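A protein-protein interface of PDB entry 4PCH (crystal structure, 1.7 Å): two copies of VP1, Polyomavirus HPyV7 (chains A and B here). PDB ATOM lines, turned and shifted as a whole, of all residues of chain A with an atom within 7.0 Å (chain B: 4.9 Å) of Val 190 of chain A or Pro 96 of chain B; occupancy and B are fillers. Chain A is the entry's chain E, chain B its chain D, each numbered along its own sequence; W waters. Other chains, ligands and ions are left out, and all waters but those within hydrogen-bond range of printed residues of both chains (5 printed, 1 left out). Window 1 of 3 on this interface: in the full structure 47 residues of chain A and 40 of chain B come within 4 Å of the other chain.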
ATOM      1  N   TYR A  61       7.740   8.895   8.958  1.00  0.00           N
ATOM      2  CA  TYR A  61       9.153   9.178   8.745  1.00  0.00           C
ATOM      3  C   TYR A  61       9.945   7.869   8.777  1.00  0.00           C
ATOM      4  O   TYR A  61       9.666   6.969   9.601  1.00  0.00           O
ATOM      5  CB  TYR A  61       9.695  10.130   9.805  1.00  0.00           C
ATOM      6  CG  TYR A  61       9.228  11.565   9.692  1.00  0.00           C
ATOM      7  CD1 TYR A  61       9.784  12.432   8.747  1.00  0.00           C
ATOM      8  CD2 TYR A  61       8.260  12.073  10.542  1.00  0.00           C
ATOM      9  CE1 TYR A  61       9.362  13.747   8.647  1.00  0.00           C
ATOM     10  CE2 TYR A  61       7.839  13.394  10.454  1.00  0.00           C
ATOM     11  CZ  TYR A  61       8.403  14.233   9.504  1.00  0.00           C
ATOM     12  OH  TYR A  61       7.970  15.541   9.408  1.00  0.00           O
ATOM     13  N   THR A 116      -1.219  14.987  -3.405  1.00  0.00           N
ATOM     14  CA  THR A 116      -0.424  15.669  -2.383  1.00  0.00           C
ATOM     15  C   THR A 116       0.911  14.947  -2.161  1.00  0.00           C
ATOM     16  O   THR A 116       0.976  13.712  -2.190  1.00  0.00           O
ATOM     17  CB  THR A 116      -1.308  15.827  -1.124  1.00  0.00           C
ATOM     18  OG1 THR A 116      -2.290  16.840  -1.385  1.00  0.00           O
ATOM     19  CG2 THR A 116      -0.509  16.188   0.117  1.00  0.00           C
ATOM     20  N   GLN A 117       1.967  15.736  -1.909  1.00  0.00           N
ATOM     21  CA  GLN A 117       3.318  15.229  -1.858  1.00  0.00           C
ATOM     22  C   GLN A 117       4.114  15.812  -0.706  1.00  0.00           C
ATOM     23  O   GLN A 117       3.834  16.916  -0.221  1.00  0.00           O
ATOM     24  CB  GLN A 117       4.086  15.558  -3.148  1.00  0.00           C
ATOM     25  CG  GLN A 117       3.401  15.080  -4.430  1.00  0.00           C
ATOM     26  CD  GLN A 117       3.791  15.877  -5.652  1.00  0.00           C
ATOM     27  OE1 GLN A 117       4.975  16.043  -5.969  1.00  0.00           O
ATOM     28  NE2 GLN A 117       2.782  16.373  -6.371  1.00  0.00           N
ATOM     29  N   LEU A 118       5.132  15.062  -0.306  1.00  0.00           N
ATOM     30  CA  LEU A 118       6.119  15.553   0.626  1.00  0.00           C
ATOM     31  C   LEU A 118       7.463  14.936   0.317  1.00  0.00           C
ATOM     32  O   LEU A 118       7.559  13.722   0.209  1.00  0.00           O
ATOM     33  CB  LEU A 118       5.740  15.180   2.049  1.00  0.00           C
ATOM     34  CG  LEU A 118       6.831  15.413   3.106  1.00  0.00           C
ATOM     35  CD1 LEU A 118       7.078  16.894   3.299  1.00  0.00           C
ATOM     36  CD2 LEU A 118       6.464  14.725   4.409  1.00  0.00           C
ATOM     37  N   TYR A 119       8.482  15.779   0.204  1.00  0.00           N
ATOM     38  CA  TYR A 119       9.846  15.312   0.046  1.00  0.00           C
ATOM     39  C   TYR A 119      10.658  15.940   1.156  1.00  0.00           C
ATOM     40  O   TYR A 119      10.797  17.160   1.189  1.00  0.00           O
ATOM     41  CB  TYR A 119      10.379  15.742  -1.312  1.00  0.00           C
ATOM     42  CG  TYR A 119       9.442  15.319  -2.406  1.00  0.00           C
ATOM     43  CD1 TYR A 119       9.428  13.999  -2.861  1.00  0.00           C
ATOM     44  CD2 TYR A 119       8.565  16.227  -2.978  1.00  0.00           C
ATOM     45  CE1 TYR A 119       8.547  13.588  -3.857  1.00  0.00           C
ATOM     46  CE2 TYR A 119       7.674  15.830  -3.988  1.00  0.00           C
ATOM     47  CZ  TYR A 119       7.674  14.508  -4.421  1.00  0.00           C
ATOM     48  OH  TYR A 119       6.800  14.083  -5.392  1.00  0.00           O
ATOM     49  N   PRO A 135      -4.291  19.280  12.331  1.00  0.00           N
ATOM     50  CA  PRO A 135      -4.844  20.399  11.597  1.00  0.00           C
ATOM     51  C   PRO A 135      -6.327  20.603  11.874  1.00  0.00           C
ATOM     52  O   PRO A 135      -6.864  21.655  11.557  1.00  0.00           O
ATOM     53  CB  PRO A 135      -4.590  20.009  10.134  1.00  0.00           C
ATOM     54  CG  PRO A 135      -4.611  18.531  10.137  1.00  0.00           C
ATOM     55  CD  PRO A 135      -3.899  18.184  11.419  1.00  0.00           C
ATOM     56  N   VAL A 171       3.807  11.601   8.865  1.00  0.00           N
ATOM     57  CA  VAL A 171       4.308  12.862   8.339  1.00  0.00           C
ATOM     58  C   VAL A 171       3.186  13.886   8.224  1.00  0.00           C
ATOM     59  O   VAL A 171       3.459  15.085   8.160  1.00  0.00           O
ATOM     60  CB  VAL A 171       5.014  12.684   6.977  1.00  0.00           C
ATOM     61  CG1 VAL A 171       6.170  11.680   7.076  1.00  0.00           C
ATOM     62  CG2 VAL A 171       4.025  12.252   5.898  1.00  0.00           C
ATOM     63  N   GLU A 172       1.935  13.427   8.201  1.00  0.00           N
ATOM     64  CA  GLU A 172       0.792  14.334   8.203  1.00  0.00           C
ATOM     65  C   GLU A 172       0.604  15.076   9.544  1.00  0.00           C
ATOM     66  O   GLU A 172      -0.112  16.073   9.605  1.00  0.00           O
ATOM     67  CB  GLU A 172      -0.508  13.558   7.850  1.00  0.00           C
ATOM     68  CG  GLU A 172      -0.599  13.076   6.409  1.00  0.00           C
ATOM     69  CD  GLU A 172      -1.569  11.913   6.262  1.00  0.00           C
ATOM     70  OE1 GLU A 172      -2.770  12.100   6.555  1.00  0.00           O
ATOM     71  OE2 GLU A 172      -1.132  10.800   5.892  1.00  0.00           O
ATOM     72  N   LEU A 173       1.260  14.607  10.613  1.00  0.00           N
ATOM     73  CA  LEU A 173       0.983  15.066  11.976  1.00  0.00           C
ATOM     74  C   LEU A 173       2.184  15.690  12.699  1.00  0.00           C
ATOM     75  O   LEU A 173       2.014  16.260  13.775  1.00  0.00           O
ATOM     76  CB  LEU A 173       0.482  13.895  12.818  1.00  0.00           C
ATOM     77  CG  LEU A 173      -0.729  13.158  12.237  1.00  0.00           C
ATOM     78  CD1 LEU A 173      -1.119  11.988  13.133  1.00  0.00           C
ATOM     79  CD2 LEU A 173      -1.892  14.105  12.037  1.00  0.00           C
ATOM     80  N   TRP A 174       3.373  15.547  12.136  1.00  0.00           N
ATOM     81  CA  TRP A 174       4.614  15.951  12.803  1.00  0.00           C
ATOM     82  C   TRP A 174       5.502  16.749  11.852  1.00  0.00           C
ATOM     83  O   TRP A 174       5.891  16.261  10.793  1.00  0.00           O
ATOM     84  CB  TRP A 174       5.363  14.721  13.302  1.00  0.00           C
ATOM     85  CG  TRP A 174       4.624  13.967  14.360  1.00  0.00           C
ATOM     86  CD1 TRP A 174       3.794  12.905  14.171  1.00  0.00           C
ATOM     87  CD2 TRP A 174       4.612  14.236  15.773  1.00  0.00           C
ATOM     88  NE1 TRP A 174       3.286  12.473  15.376  1.00  0.00           N
ATOM     89  CE2 TRP A 174       3.767  13.276  16.374  1.00  0.00           C
ATOM     90  CE3 TRP A 174       5.231  15.190  16.585  1.00  0.00           C
ATOM     91  CZ2 TRP A 174       3.539  13.236  17.756  1.00  0.00           C
ATOM     92  CZ3 TRP A 174       5.002  15.143  17.966  1.00  0.00           C
ATOM     93  CH2 TRP A 174       4.154  14.183  18.525  1.00  0.00           C
ATOM     94  N   VAL A 175       5.851  17.954  12.272  1.00  0.00           N
ATOM     95  CA  VAL A 175       6.629  18.893  11.469  1.00  0.00           C
ATOM     96  C   VAL A 175       7.984  19.145  12.131  1.00  0.00           C
ATOM     97  O   VAL A 175       8.048  19.291  13.353  1.00  0.00           O
ATOM     98  CB  VAL A 175       5.901  20.234  11.379  1.00  0.00           C
ATOM     99  CG1 VAL A 175       6.670  21.190  10.477  1.00  0.00           C
ATOM    100  CG2 VAL A 175       4.475  20.032  10.871  1.00  0.00           C
ATOM    101  N   GLY A 188      12.423  20.328   3.546  1.00  0.00           N
ATOM    102  CA  GLY A 188      11.178  19.729   3.110  1.00  0.00           C
ATOM    103  C   GLY A 188      10.403  20.551   2.097  1.00  0.00           C
ATOM    104  O   GLY A 188      10.469  21.772   2.074  1.00  0.00           O
ATOM    105  N   ARG A 189       9.663  19.848   1.249  1.00  0.00           N
ATOM    106  CA  ARG A 189       8.800  20.466   0.237  1.00  0.00           C
ATOM    107  C   ARG A 189       7.452  19.747   0.241  1.00  0.00           C
ATOM    108  O   ARG A 189       7.394  18.512   0.152  1.00  0.00           O
ATOM    109  CB  ARG A 189       9.456  20.387  -1.152  1.00  0.00           C
ATOM    110  CG  ARG A 189       8.641  21.004  -2.272  1.00  0.00           C
ATOM    111  CD  ARG A 189       9.507  21.261  -3.493  1.00  0.00           C
ATOM    112  NE  ARG A 189       9.683  20.057  -4.299  1.00  0.00           N
ATOM    113  CZ  ARG A 189      10.719  19.231  -4.236  1.00  0.00           C
ATOM    114  NH1 ARG A 189      10.740  18.179  -5.032  1.00  0.00           N
ATOM    115  NH2 ARG A 189      11.721  19.440  -3.387  1.00  0.00           N
ATOM    116  N   VAL A 190       6.382  20.522   0.369  1.00  0.00           N
ATOM    117  CA  VAL A 190       5.005  19.975   0.394  1.00  0.00           C
ATOM    118  C   VAL A 190       4.278  20.493  -0.850  1.00  0.00           C
ATOM    119  O   VAL A 190       4.398  21.666  -1.186  1.00  0.00           O
ATOM    120  CB  VAL A 190       4.250  20.438   1.655  1.00  0.00           C
ATOM    121  CG1 VAL A 190       2.773  19.984   1.646  1.00  0.00           C
ATOM    122  CG2 VAL A 190       4.967  19.966   2.913  1.00  0.00           C
ATOM    123  N   VAL A 191       3.532  19.613  -1.521  1.00  0.00           N
ATOM    124  CA  VAL A 191       2.701  19.992  -2.636  1.00  0.00           C
ATOM    125  C   VAL A 191       1.280  19.594  -2.268  1.00  0.00           C
ATOM    126  O   VAL A 191       1.057  18.477  -1.794  1.00  0.00           O
ATOM    127  CB  VAL A 191       3.138  19.298  -3.943  1.00  0.00           C
ATOM    128  CG1 VAL A 191       2.258  19.724  -5.108  1.00  0.00           C
ATOM    129  CG2 VAL A 191       4.585  19.640  -4.274  1.00  0.00           C
ATOM    130  N   GLY A 192       0.335  20.512  -2.436  1.00  0.00           N
ATOM    131  CA  GLY A 192      -1.083  20.207  -2.180  1.00  0.00           C
ATOM    132  C   GLY A 192      -1.876  19.679  -3.369  1.00  0.00           C
ATOM    133  O   GLY A 192      -1.314  19.216  -4.359  1.00  0.00           O
ATOM    134  N   MET A 232       6.695  11.102  -0.067  1.00  0.00           N
ATOM    135  CA  MET A 232       5.375  10.791  -0.585  1.00  0.00           C
ATOM    136  C   MET A 232       5.263  11.428  -1.966  1.00  0.00           C
ATOM    137  O   MET A 232       5.206  12.645  -2.104  1.00  0.00           O
ATOM    138  CB  MET A 232       4.277  11.297   0.352  1.00  0.00           C
ATOM    139  CG  MET A 232       2.890  11.078  -0.206  1.00  0.00           C
ATOM    140  SD  MET A 232       1.570  11.369   1.004  1.00  0.00           S
ATOM    141  CE  MET A 232       1.802  13.119   1.247  1.00  0.00           C
ATOM    142  N   PHE B  94       4.315  23.620   8.140  1.00  0.00           N
ATOM    143  CA  PHE B  94       3.172  23.031   7.473  1.00  0.00           C
ATOM    144  C   PHE B  94       3.448  21.567   7.163  1.00  0.00           C
ATOM    145  O   PHE B  94       4.598  21.173   6.944  1.00  0.00           O
ATOM    146  CB  PHE B  94       2.866  23.776   6.166  1.00  0.00           C
ATOM    147  CG  PHE B  94       1.496  23.512   5.642  1.00  0.00           C
ATOM    148  CD1 PHE B  94       0.384  23.860   6.394  1.00  0.00           C
ATOM    149  CD2 PHE B  94       1.305  22.922   4.410  1.00  0.00           C
ATOM    150  CE1 PHE B  94      -0.889  23.620   5.935  1.00  0.00           C
ATOM    151  CE2 PHE B  94       0.016  22.681   3.943  1.00  0.00           C
ATOM    152  CZ  PHE B  94      -1.065  23.024   4.704  1.00  0.00           C
ATOM    153  N   ALA B  95       2.379  20.773   7.177  1.00  0.00           N
ATOM    154  CA  ALA B  95       2.411  19.353   6.849  1.00  0.00           C
ATOM    155  C   ALA B  95       1.476  19.048   5.670  1.00  0.00           C
ATOM    156  O   ALA B  95       0.512  19.791   5.404  1.00  0.00           O
ATOM    157  CB  ALA B  95       1.983  18.538   8.041  1.00  0.00           C
ATOM    158  N   PRO B  96       1.737  17.935   4.972  1.00  0.00           N
ATOM    159  CA  PRO B  96       0.788  17.558   3.900  1.00  0.00           C
ATOM    160  C   PRO B  96      -0.608  17.295   4.462  1.00  0.00           C
ATOM    161  O   PRO B  96      -0.746  16.672   5.492  1.00  0.00           O
ATOM    162  CB  PRO B  96       1.400  16.259   3.331  1.00  0.00           C
ATOM    163  CG  PRO B  96       2.271  15.744   4.422  1.00  0.00           C
ATOM    164  CD  PRO B  96       2.842  16.973   5.071  1.00  0.00           C
ATOM    165  N   GLN B  97      -1.645  17.777   3.778  1.00  0.00           N
ATOM    166  CA  GLN B  97      -3.020  17.602   4.246  1.00  0.00           C
ATOM    167  C   GLN B  97      -3.689  16.526   3.404  1.00  0.00           C
ATOM    168  O   GLN B  97      -3.754  16.652   2.188  1.00  0.00           O
ATOM    169  CB  GLN B  97      -3.821  18.900   4.115  1.00  0.00           C
ATOM    170  CG  GLN B  97      -3.217  20.087   4.835  1.00  0.00           C
ATOM    171  CD  GLN B  97      -3.156  19.884   6.347  1.00  0.00           C
ATOM    172  OE1 GLN B  97      -4.145  19.488   6.984  1.00  0.00           O
ATOM    173  NE2 GLN B  97      -1.992  20.129   6.922  1.00  0.00           N
ATOM    174  N   MET B  98      -4.136  15.455   4.058  1.00  0.00           N
ATOM    175  CA  MET B  98      -4.690  14.287   3.377  1.00  0.00           C
ATOM    176  C   MET B  98      -6.095  14.009   3.923  1.00  0.00           C
ATOM    177  O   MET B  98      -7.052  14.674   3.539  1.00  0.00           O
ATOM    178  CB  MET B  98      -3.751  13.094   3.569  1.00  0.00           C
ATOM    179  CG  MET B  98      -2.344  13.320   3.030  1.00  0.00           C
ATOM    180  SD  MET B  98      -2.192  12.966   1.270  1.00  0.00           S
ATOM    181  CE  MET B  98      -2.338  11.179   1.272  1.00  0.00           C
ATOM    182  N   PRO B 198      -0.977  24.304  -3.936  1.00  0.00           N
ATOM    183  CA  PRO B 198       0.104  25.038  -3.295  1.00  0.00           C
ATOM    184  C   PRO B 198       1.412  24.245  -3.251  1.00  0.00           C
ATOM    185  O   PRO B 198       1.394  22.998  -3.232  1.00  0.00           O
ATOM    186  CB  PRO B 198      -0.425  25.260  -1.903  1.00  0.00           C
ATOM    187  CG  PRO B 198      -1.222  24.020  -1.609  1.00  0.00           C
ATOM    188  CD  PRO B 198      -1.896  23.725  -2.940  1.00  0.00           C
ATOM    189  N   VAL B 199       2.531  24.977  -3.249  1.00  0.00           N
ATOM    190  CA  VAL B 199       3.854  24.371  -3.087  1.00  0.00           C
ATOM    191  C   VAL B 199       4.533  25.163  -1.985  1.00  0.00           C
ATOM    192  O   VAL B 199       4.691  26.377  -2.118  1.00  0.00           O
ATOM    193  CB  VAL B 199       4.688  24.441  -4.380  1.00  0.00           C
ATOM    194  CG1 VAL B 199       6.080  23.840  -4.168  1.00  0.00           C
ATOM    195  CG2 VAL B 199       3.971  23.746  -5.522  1.00  0.00           C
ATOM    196  N   VAL B 200       4.883  24.478  -0.908  1.00  0.00           N
ATOM    197  CA  VAL B 200       5.500  25.088   0.293  1.00  0.00           C
ATOM    198  C   VAL B 200       6.852  24.412   0.508  1.00  0.00           C
ATOM    199  O   VAL B 200       6.928  23.191   0.544  1.00  0.00           O
ATOM    200  CB  VAL B 200       4.579  24.881   1.521  1.00  0.00           C
ATOM    201  CG1 VAL B 200       5.296  25.111   2.850  1.00  0.00           C
ATOM    202  CG2 VAL B 200       3.375  25.806   1.410  1.00  0.00           C
ATOM    203  N   TYR B 202      10.490  24.442   3.047  1.00  0.00           N
ATOM    204  CA  TYR B 202      11.050  24.874   4.331  1.00  0.00           C
ATOM    205  C   TYR B 202      12.324  24.117   4.630  1.00  0.00           C
ATOM    206  O   TYR B 202      12.605  23.069   4.059  1.00  0.00           O
ATOM    207  CB  TYR B 202      10.052  24.664   5.479  1.00  0.00           C
ATOM    208  CG  TYR B 202       9.636  23.221   5.658  1.00  0.00           C
ATOM    209  CD1 TYR B 202      10.373  22.348   6.439  1.00  0.00           C
ATOM    210  CD2 TYR B 202       8.488  22.716   5.025  1.00  0.00           C
ATOM    211  CE1 TYR B 202       9.998  21.024   6.584  1.00  0.00           C
ATOM    212  CE2 TYR B 202       8.114  21.397   5.175  1.00  0.00           C
ATOM    213  CZ  TYR B 202       8.858  20.554   5.948  1.00  0.00           C
ATOM    214  OH  TYR B 202       8.511  19.238   6.094  1.00  0.00           O
HETATM  215  O   HOH W   1       8.692  18.073   8.700  1.00  0.00           O
HETATM  216  O   HOH W   2      -2.377  16.567   7.930  1.00  0.00           O
HETATM  217  O   HOH W   3      -3.045  18.684   0.371  1.00  0.00           O
HETATM  218  O   HOH W   4      -4.179  14.680   6.758  1.00  0.00           O
HETATM  219  O   HOH W   5      -4.613  15.007  -0.768  1.00  0.00           O
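Thr 116 of chain A touches Pro 96 of chain B.
Tyr 202 of chain B touches Leu 118 of chain A.
Val 171 of chain A touches Pro 96 of chain B.
Ala 95 of chain B touches Glu 172 of chain A (CB to O, 3.6 Å).
CG of Glu 172 of chain A touches O of Pro 96 of chain B, 3.7 Å away.
Glu 172 of chain A touches Met 98 of chain B.
Val 200 of chain B touches Arg 189 of chain A.
Val 190 of chain A touches Pro 96 of chain B.
O of Pro 198 of chain B touches CA of Val 191 of chain A, 3.3 Å away.
CE of Met 232 of chain A touches CB of Pro 96 of chain B (3.8 Å).
The backbone carbonyl oxygen of Pro 198 of chain B is in hydrogen-bond range of the backbone NH of Gly 192 of chain A (2.8 Å).
The backbone carbonyl oxygen of Val 200 of chain B is in hydrogen-bond range of the backbone NH of Val 190 of chain A.
O of Tyr 202 of chain B sits at hydrogen-bond distance from N of Gly 188 of chain A, at 2.8 Å.
Printed residues of chain B within 4 Å of Glu 172 of chain A: Ala 95 (3.6 Å), Pro 96 (3.7 Å) and Met 98 (3.3 Å).
Val 190 of chain A touches just these residues of chain B: Pro 96 (3.9 Å), Pro 198 (3.9 Å), Val 199 (3.4 Å) and Val 200 (2.7 Å).
Pro 96 of chain B touches just these residues of chain A: Thr 116, Val 171, Glu 172, Val 190 and Met 232.
Of the printed residues of chain A, Gln 97 of chain B touches Thr 116 and Pro 135.
The nearest residue of chain B that does not touch Val 190 of chain A is Tyr 202 of chain B (4.1 Å).
The nearest residue of chain A that does not touch Pro 96 of chain B is Leu 118 of chain A (4.2 Å).
O of Ala 95 of chain B is in hydrogen-bond range of NE2 of Gln 97 of chain B (2.9 Å).
The backbone NH (N) of Gln 117 of chain A lies within hydrogen-bond range of the backbone carbonyl oxygen (O) of Val 191 of chain A (2.9 Å).
O of Leu 118 of chain A is in hydrogen-bond range of N of Met 232 of chain A, 2.8 Å away.
O of Tyr 119 of chain A sits at hydrogen-bond distance from N of Arg 189 of chain A.
No position is printed for both chains.
Water W3 bridges the side-chain hydroxyl (OG1) of Thr 116 of chain A (2.7 Å) and the backbone carbonyl oxygen (O) of Gln 97 of chain B (2.8 Å).
Water W1 bridges the side-chain hydroxyl of Tyr 61 of chain A (2.7 Å) and the side-chain hydroxyl of Tyr 202 of chain B (2.9 Å).
Water W4 bridges N of Met 98 of chain B and OE1 of Glu 172 of chain A.
Water W2 lies within hydrogen-bond range of the backbone carbonyl oxygen of Glu 172 of chain A (2.9 Å) and the backbone carbonyl oxygen of Pro 96 of chain B (2.9 Å).
Water W5 lies within hydrogen-bond range of the side-chain hydroxyl of Thr 116 of chain A (3.0 Å), the backbone carbonyl oxygen of Gln 97 of chain B (3.5 Å) and the side-chain sulfur of Met 98 of chain B (3.8 Å).
Hydrophobic or aromatic side chains of chain B within 4 Å of the printed part of chain A: Ala 95, Pro 96, Met 98, Pro 198 and Tyr 202.
Hydrophobic or aromatic side chains of chain A within 4 Å of the printed part of chain B: Leu 118, Pro 135, Val 190, Val 191 and Met 232.
Among the printed residues, 20 pairs touch across the chains.
Among the printed residues, no Asp or Glu carboxylate lies within 4 Å of a Lys or Arg side-chain nitrogen of the other chain.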
